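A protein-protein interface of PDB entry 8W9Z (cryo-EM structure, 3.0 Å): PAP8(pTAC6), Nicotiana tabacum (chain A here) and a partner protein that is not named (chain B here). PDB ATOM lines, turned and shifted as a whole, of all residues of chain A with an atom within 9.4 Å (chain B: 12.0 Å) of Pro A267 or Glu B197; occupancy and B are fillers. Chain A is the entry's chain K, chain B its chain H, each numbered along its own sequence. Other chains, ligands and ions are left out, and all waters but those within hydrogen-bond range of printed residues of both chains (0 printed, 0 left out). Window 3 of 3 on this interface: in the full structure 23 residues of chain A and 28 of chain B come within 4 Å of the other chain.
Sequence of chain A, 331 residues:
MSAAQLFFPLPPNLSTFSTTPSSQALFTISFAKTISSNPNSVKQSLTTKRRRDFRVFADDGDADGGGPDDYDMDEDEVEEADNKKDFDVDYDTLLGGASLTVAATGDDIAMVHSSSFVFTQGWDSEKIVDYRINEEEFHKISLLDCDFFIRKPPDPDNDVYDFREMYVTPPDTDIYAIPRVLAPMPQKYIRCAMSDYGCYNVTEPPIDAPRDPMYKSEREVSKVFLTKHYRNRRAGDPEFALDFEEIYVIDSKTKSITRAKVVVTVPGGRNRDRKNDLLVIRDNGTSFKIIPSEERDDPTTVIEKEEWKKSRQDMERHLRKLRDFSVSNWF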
ATOM      1  N   VAL A 264       3.721  31.313  -9.811  1.00  0.00           N
ATOM      2  CA  VAL A 264       4.804  30.640 -10.519  1.00  0.00           C
ATOM      3  C   VAL A 264       5.179  29.384  -9.738  1.00  0.00           C
ATOM      4  O   VAL A 264       5.796  29.464  -8.674  1.00  0.00           O
ATOM      5  CB  VAL A 264       6.015  31.563 -10.701  1.00  0.00           C
ATOM      6  CG1 VAL A 264       7.129  30.834 -11.431  1.00  0.00           C
ATOM      7  CG2 VAL A 264       5.612  32.822 -11.452  1.00  0.00           C
ATOM      8  N   THR A 265       4.806  28.223 -10.267  1.00  0.00           N
ATOM      9  CA  THR A 265       5.108  26.929  -9.657  1.00  0.00           C
ATOM     10  C   THR A 265       5.917  26.118 -10.663  1.00  0.00           C
ATOM     11  O   THR A 265       5.361  25.335 -11.436  1.00  0.00           O
ATOM     12  CB  THR A 265       3.834  26.191  -9.246  1.00  0.00           C
ATOM     13  OG1 THR A 265       3.023  25.954 -10.404  1.00  0.00           O
ATOM     14  CG2 THR A 265       3.043  27.011  -8.239  1.00  0.00           C
ATOM     15  N   VAL A 266       7.232  26.305 -10.646  1.00  0.00           N
ATOM     16  CA  VAL A 266       8.133  25.565 -11.524  1.00  0.00           C
ATOM     17  C   VAL A 266       9.527  25.560 -10.907  1.00  0.00           C
ATOM     18  O   VAL A 266      10.025  26.615 -10.486  1.00  0.00           O
ATOM     19  CB  VAL A 266       8.142  26.158 -12.944  1.00  0.00           C
ATOM     20  CG1 VAL A 266       8.365  27.662 -12.904  1.00  0.00           C
ATOM     21  CG2 VAL A 266       9.198  25.477 -13.801  1.00  0.00           C
ATOM     22  N   PRO A 267      10.182  24.403 -10.807  1.00  0.00           N
ATOM     23  CA  PRO A 267      11.532  24.373 -10.233  1.00  0.00           C
ATOM     24  C   PRO A 267      12.536  25.066 -11.139  1.00  0.00           C
ATOM     25  O   PRO A 267      12.517  24.902 -12.361  1.00  0.00           O
ATOM     26  CB  PRO A 267      11.833  22.874 -10.109  1.00  0.00           C
ATOM     27  CG  PRO A 267      10.494  22.200 -10.166  1.00  0.00           C
ATOM     28  CD  PRO A 267       9.661  23.053 -11.069  1.00  0.00           C
ATOM     29  N   GLY A 268      13.419  25.847 -10.524  1.00  0.00           N
ATOM     30  CA  GLY A 268      14.449  26.549 -11.265  1.00  0.00           C
ATOM     31  C   GLY A 268      14.628  27.990 -10.835  1.00  0.00           C
ATOM     32  O   GLY A 268      15.738  28.527 -10.891  1.00  0.00           O
ATOM     33  N   GLY A 269      13.541  28.626 -10.401  1.00  0.00           N
ATOM     34  CA  GLY A 269      13.626  30.010  -9.980  1.00  0.00           C
ATOM     35  C   GLY A 269      13.889  30.944 -11.149  1.00  0.00           C
ATOM     36  O   GLY A 269      13.441  30.723 -12.279  1.00  0.00           O
ATOM     37  N   ARG A 270      14.637  32.013 -10.868  1.00  0.00           N
ATOM     38  CA  ARG A 270      14.968  32.983 -11.905  1.00  0.00           C
ATOM     39  C   ARG A 270      16.067  32.479 -12.831  1.00  0.00           C
ATOM     40  O   ARG A 270      16.147  32.917 -13.984  1.00  0.00           O
ATOM     41  CB  ARG A 270      15.386  34.315 -11.276  1.00  0.00           C
ATOM     42  CG  ARG A 270      14.237  35.145 -10.715  1.00  0.00           C
ATOM     43  CD  ARG A 270      13.801  34.665  -9.338  1.00  0.00           C
ATOM     44  NE  ARG A 270      12.692  35.454  -8.811  1.00  0.00           N
ATOM     45  CZ  ARG A 270      12.838  36.557  -8.085  1.00  0.00           C
ATOM     46  NH1 ARG A 270      14.052  37.008  -7.798  1.00  0.00           N
ATOM     47  NH2 ARG A 270      11.771  37.211  -7.647  1.00  0.00           N
ATOM     48  N   ASN A 271      16.916  31.567 -12.351  1.00  0.00           N
ATOM     49  CA  ASN A 271      17.980  31.025 -13.190  1.00  0.00           C
ATOM     50  C   ASN A 271      17.441  30.139 -14.304  1.00  0.00           C
ATOM     51  O   ASN A 271      18.136  29.932 -15.305  1.00  0.00           O
ATOM     52  CB  ASN A 271      18.974  30.237 -12.335  1.00  0.00           C
ATOM     53  CG  ASN A 271      19.636  31.094 -11.274  1.00  0.00           C
ATOM     54  OD1 ASN A 271      19.824  32.296 -11.458  1.00  0.00           O
ATOM     55  ND2 ASN A 271      19.996  30.476 -10.155  1.00  0.00           N
ATOM     56  N   ARG A 272      16.229  29.611 -14.153  1.00  0.00           N
ATOM     57  CA  ARG A 272      15.623  28.799 -15.200  1.00  0.00           C
ATOM     58  C   ARG A 272      15.300  29.660 -16.414  1.00  0.00           C
ATOM     59  O   ARG A 272      14.727  30.747 -16.285  1.00  0.00           O
ATOM     60  CB  ARG A 272      14.356  28.127 -14.675  1.00  0.00           C
ATOM     61  CG  ARG A 272      13.526  27.445 -15.747  1.00  0.00           C
ATOM     62  CD  ARG A 272      12.121  27.161 -15.244  1.00  0.00           C
ATOM     63  NE  ARG A 272      11.505  28.353 -14.671  1.00  0.00           N
ATOM     64  CZ  ARG A 272      10.900  29.300 -15.381  1.00  0.00           C
ATOM     65  NH1 ARG A 272      10.830  29.197 -16.701  1.00  0.00           N
ATOM     66  NH2 ARG A 272      10.368  30.351 -14.774  1.00  0.00           N
ATOM     67  N   ASP A 273      15.672  29.175 -17.596  1.00  0.00           N
ATOM     68  CA  ASP A 273      15.383  29.897 -18.827  1.00  0.00           C
ATOM     69  C   ASP A 273      13.881  29.924 -19.082  1.00  0.00           C
ATOM     70  O   ASP A 273      13.196  28.907 -18.939  1.00  0.00           O
ATOM     71  CB  ASP A 273      16.114  29.254 -20.005  1.00  0.00           C
ATOM     72  CG  ASP A 273      15.921  27.750 -20.062  1.00  0.00           C
ATOM     73  OD1 ASP A 273      15.412  27.174 -19.077  1.00  0.00           O
ATOM     74  OD2 ASP A 273      16.280  27.143 -21.093  1.00  0.00           O
ATOM     75  N   ASN A 276      10.597  27.279 -21.463  1.00  0.00           N
ATOM     76  CA  ASN A 276       9.768  26.110 -21.185  1.00  0.00           C
ATOM     77  C   ASN A 276       8.774  26.519 -20.102  1.00  0.00           C
ATOM     78  O   ASN A 276       8.998  26.276 -18.914  1.00  0.00           O
ATOM     79  CB  ASN A 276      10.627  24.921 -20.753  1.00  0.00           C
ATOM     80  CG  ASN A 276       9.841  23.630 -20.675  1.00  0.00           C
ATOM     81  OD1 ASN A 276       8.867  23.438 -21.402  1.00  0.00           O
ATOM     82  ND2 ASN A 276      10.260  22.734 -19.789  1.00  0.00           N
ATOM     83  N   ASP A 277       7.671  27.137 -20.521  1.00  0.00           N
ATOM     84  CA  ASP A 277       6.647  27.609 -19.600  1.00  0.00           C
ATOM     85  C   ASP A 277       5.288  27.492 -20.271  1.00  0.00           C
ATOM     86  O   ASP A 277       5.186  27.360 -21.493  1.00  0.00           O
ATOM     87  CB  ASP A 277       6.899  29.056 -19.160  1.00  0.00           C
ATOM     88  CG  ASP A 277       8.027  29.175 -18.156  1.00  0.00           C
ATOM     89  OD1 ASP A 277       8.105  28.328 -17.242  1.00  0.00           O
ATOM     90  OD2 ASP A 277       8.836  30.118 -18.281  1.00  0.00           O
ATOM     91  N   LYS A 289      -1.444  30.289 -13.472  1.00  0.00           N
ATOM     92  CA  LYS A 289      -0.418  29.372 -12.993  1.00  0.00           C
ATOM     93  C   LYS A 289       0.590  29.134 -14.105  1.00  0.00           C
ATOM     94  O   LYS A 289       0.204  28.874 -15.248  1.00  0.00           O
ATOM     95  CB  LYS A 289      -1.023  28.040 -12.539  1.00  0.00           C
ATOM     96  CG  LYS A 289      -1.904  28.135 -11.305  1.00  0.00           C
ATOM     97  CD  LYS A 289      -2.465  26.774 -10.924  1.00  0.00           C
ATOM     98  CE  LYS A 289      -1.354  25.781 -10.632  1.00  0.00           C
ATOM     99  NZ  LYS A 289      -0.490  26.230  -9.505  1.00  0.00           N
ATOM    100  N   ILE A 290       1.873  29.219 -13.769  1.00  0.00           N
ATOM    101  CA  ILE A 290       2.954  28.981 -14.718  1.00  0.00           C
ATOM    102  C   ILE A 290       3.521  27.595 -14.448  1.00  0.00           C
ATOM    103  O   ILE A 290       4.068  27.336 -13.369  1.00  0.00           O
ATOM    104  CB  ILE A 290       4.047  30.057 -14.616  1.00  0.00           C
ATOM    105  CG1 ILE A 290       3.560  31.390 -15.192  1.00  0.00           C
ATOM    106  CG2 ILE A 290       5.306  29.606 -15.338  1.00  0.00           C
ATOM    107  CD1 ILE A 290       2.783  32.250 -14.213  1.00  0.00           C
ATOM    108  N   ILE A 291       3.383  26.701 -15.422  1.00  0.00           N
ATOM    109  CA  ILE A 291       3.859  25.326 -15.287  1.00  0.00           C
ATOM    110  C   ILE A 291       4.681  24.981 -16.522  1.00  0.00           C
ATOM    111  O   ILE A 291       4.500  25.581 -17.594  1.00  0.00           O
ATOM    112  CB  ILE A 291       2.689  24.330 -15.104  1.00  0.00           C
ATOM    113  CG1 ILE A 291       1.756  24.368 -16.314  1.00  0.00           C
ATOM    114  CG2 ILE A 291       1.924  24.629 -13.824  1.00  0.00           C
ATOM    115  CD1 ILE A 291       0.620  23.374 -16.235  1.00  0.00           C
ATOM    116  N   PRO A 292       5.604  24.027 -16.403  1.00  0.00           N
ATOM    117  CA  PRO A 292       6.390  23.620 -17.573  1.00  0.00           C
ATOM    118  C   PRO A 292       5.518  22.976 -18.640  1.00  0.00           C
ATOM    119  O   PRO A 292       4.436  22.451 -18.371  1.00  0.00           O
ATOM    120  CB  PRO A 292       7.399  22.618 -16.995  1.00  0.00           C
ATOM    121  CG  PRO A 292       6.788  22.154 -15.714  1.00  0.00           C
ATOM    122  CD  PRO A 292       6.042  23.335 -15.180  1.00  0.00           C
ATOM    123  N   GLU A 295       4.330  18.866 -18.450  1.00  0.00           N
ATOM    124  CA  GLU A 295       3.215  18.360 -17.660  1.00  0.00           C
ATOM    125  C   GLU A 295       1.883  18.984 -18.063  1.00  0.00           C
ATOM    126  O   GLU A 295       0.966  19.075 -17.239  1.00  0.00           O
ATOM    127  CB  GLU A 295       3.476  18.582 -16.171  1.00  0.00           C
ATOM    128  CG  GLU A 295       3.648  20.039 -15.776  1.00  0.00           C
ATOM    129  CD  GLU A 295       3.778  20.222 -14.278  1.00  0.00           C
ATOM    130  OE1 GLU A 295       3.855  19.204 -13.557  1.00  0.00           O
ATOM    131  OE2 GLU A 295       3.800  21.383 -13.817  1.00  0.00           O
ATOM    132  N   ILE B 193       3.832  34.926  -6.879  1.00  0.00           N
ATOM    133  CA  ILE B 193       4.028  33.980  -5.787  1.00  0.00           C
ATOM    134  C   ILE B 193       4.840  32.803  -6.306  1.00  0.00           C
ATOM    135  O   ILE B 193       4.482  32.196  -7.322  1.00  0.00           O
ATOM    136  CB  ILE B 193       2.687  33.494  -5.203  1.00  0.00           C
ATOM    137  CG1 ILE B 193       1.872  34.677  -4.675  1.00  0.00           C
ATOM    138  CG2 ILE B 193       2.924  32.475  -4.102  1.00  0.00           C
ATOM    139  CD1 ILE B 193       2.538  35.420  -3.539  1.00  0.00           C
ATOM    140  N   TYR B 194       5.929  32.483  -5.612  1.00  0.00           N
ATOM    141  CA  TYR B 194       6.791  31.360  -5.961  1.00  0.00           C
ATOM    142  C   TYR B 194       6.483  30.184  -5.042  1.00  0.00           C
ATOM    143  O   TYR B 194       6.664  30.281  -3.824  1.00  0.00           O
ATOM    144  CB  TYR B 194       8.265  31.749  -5.853  1.00  0.00           C
ATOM    145  CG  TYR B 194       8.791  32.523  -7.038  1.00  0.00           C
ATOM    146  CD1 TYR B 194       8.646  33.901  -7.113  1.00  0.00           C
ATOM    147  CD2 TYR B 194       9.443  31.876  -8.079  1.00  0.00           C
ATOM    148  CE1 TYR B 194       9.129  34.613  -8.196  1.00  0.00           C
ATOM    149  CE2 TYR B 194       9.930  32.577  -9.163  1.00  0.00           C
ATOM    150  CZ  TYR B 194       9.771  33.944  -9.217  1.00  0.00           C
ATOM    151  OH  TYR B 194      10.255  34.647 -10.297  1.00  0.00           O
ATOM    152  N   GLN B 195       6.019  29.081  -5.626  1.00  0.00           N
ATOM    153  CA  GLN B 195       5.725  27.856  -4.881  1.00  0.00           C
ATOM    154  C   GLN B 195       6.260  26.665  -5.662  1.00  0.00           C
ATOM    155  O   GLN B 195       5.499  25.923  -6.297  1.00  0.00           O
ATOM    156  CB  GLN B 195       4.224  27.711  -4.621  1.00  0.00           C
ATOM    157  CG  GLN B 195       3.634  28.791  -3.734  1.00  0.00           C
ATOM    158  CD  GLN B 195       2.161  28.576  -3.459  1.00  0.00           C
ATOM    159  OE1 GLN B 195       1.519  29.377  -2.779  1.00  0.00           O
ATOM    160  NE2 GLN B 195       1.613  27.488  -3.989  1.00  0.00           N
ATOM    161  N   PRO B 196       7.575  26.450  -5.640  1.00  0.00           N
ATOM    162  CA  PRO B 196       8.146  25.333  -6.401  1.00  0.00           C
ATOM    163  C   PRO B 196       7.749  23.992  -5.807  1.00  0.00           C
ATOM    164  O   PRO B 196       7.766  23.801  -4.589  1.00  0.00           O
ATOM    165  CB  PRO B 196       9.661  25.564  -6.294  1.00  0.00           C
ATOM    166  CG  PRO B 196       9.815  26.989  -5.846  1.00  0.00           C
ATOM    167  CD  PRO B 196       8.616  27.266  -4.997  1.00  0.00           C
ATOM    168  N   GLU B 197       7.388  23.059  -6.692  1.00  0.00           N
ATOM    169  CA  GLU B 197       7.030  21.691  -6.312  1.00  0.00           C
ATOM    170  C   GLU B 197       5.880  21.676  -5.304  1.00  0.00           C
ATOM    171  O   GLU B 197       5.958  21.052  -4.243  1.00  0.00           O
ATOM    172  CB  GLU B 197       8.247  20.936  -5.772  1.00  0.00           C
ATOM    173  CG  GLU B 197       9.388  20.807  -6.768  1.00  0.00           C
ATOM    174  CD  GLU B 197      10.572  20.047  -6.204  1.00  0.00           C
ATOM    175  OE1 GLU B 197      10.506  19.626  -5.030  1.00  0.00           O
ATOM    176  OE2 GLU B 197      11.569  19.872  -6.935  1.00  0.00           O
ATOM    177  N   GLN B 198       4.802  22.376  -5.646  1.00  0.00           N
ATOM    178  CA  GLN B 198       3.625  22.403  -4.788  1.00  0.00           C
ATOM    179  C   GLN B 198       2.917  21.056  -4.827  1.00  0.00           C
ATOM    180  O   GLN B 198       2.583  20.548  -5.902  1.00  0.00           O
ATOM    181  CB  GLN B 198       2.676  23.518  -5.225  1.00  0.00           C
ATOM    182  N   GLU B 199       2.686  20.476  -3.652  1.00  0.00           N
ATOM    183  CA  GLU B 199       2.053  19.172  -3.524  1.00  0.00           C
ATOM    184  C   GLU B 199       0.811  19.293  -2.654  1.00  0.00           C
ATOM    185  O   GLU B 199       0.882  19.809  -1.533  1.00  0.00           O
ATOM    186  CB  GLU B 199       3.020  18.145  -2.927  1.00  0.00           C
ATOM    187  N   GLU B 200      -0.320  18.820  -3.172  1.00  0.00           N
ATOM    188  CA  GLU B 200      -1.587  18.831  -2.449  1.00  0.00           C
ATOM    189  C   GLU B 200      -2.197  17.440  -2.520  1.00  0.00           C
ATOM    190  O   GLU B 200      -2.429  16.918  -3.616  1.00  0.00           O
ATOM    191  CB  GLU B 200      -2.548  19.872  -3.030  1.00  0.00           C
ATOM    192  N   GLU B 201      -2.455  16.844  -1.359  1.00  0.00           N
ATOM    193  CA  GLU B 201      -3.018  15.503  -1.296  1.00  0.00           C
ATOM    194  C   GLU B 201      -3.913  15.393  -0.072  1.00  0.00           C
ATOM    195  O   GLU B 201      -3.829  16.196   0.861  1.00  0.00           O
ATOM    196  CB  GLU B 201      -1.920  14.433  -1.258  1.00  0.00           C
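The backbone NH of Val A264 is in hydrogen-bond range of the backbone carbonyl oxygen of Ile B193. The backbone NH (N) of Gln B195 sits at hydrogen-bond distance from the backbone carbonyl oxygen (O) of Val A264 (3.1 Å). NE of Arg A270 is in hydrogen-bond range of OH of Tyr B194.
N of Thr A265 is in hydrogen-bond range of O of Ile A290, at 3.3 Å.
Among the printed residues, merely in contact across the chains: Val A264 with Tyr B194 (3.5 Å), Thr A265 with Gln B195 (3.3 Å) and Pro A267 with Glu B197 (3.8 Å).
Pro A267 touches just one residue of chain B: Glu B197 (3.8 Å). Glu B197 touches just one residue of chain A: Pro A267. Thr A265 touches one residue of chain B. No residue of chain B comes within 4 Å of Val A266. No residue of chain B comes within 4 Å of Gly A268. No residue of chain B comes within 4 Å of Gly A269. No residue of chain A comes within 4 Å of Pro B196. No residue of chain A comes within 4 Å of Gln B198. Of the printed residues of chain A, Ile B193 touches Val A264 (2.7 Å). Printed residues of chain B within 4 Å of Arg A270: Tyr B194. Glu A295 touches none of the printed residues of chain B. Asp A273 touches none of the printed residues of chain B. The nearest residue of chain B that does not touch Pro A267 is Pro B196 (4.5 Å).
Of the 9 printed residues of chain B, 4 touch a printed residue of chain A. Along chain B the printed residues that touch a printed residue of chain A span positions 193 to 197. Among the printed residues, 6 pairs touch across the chains.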
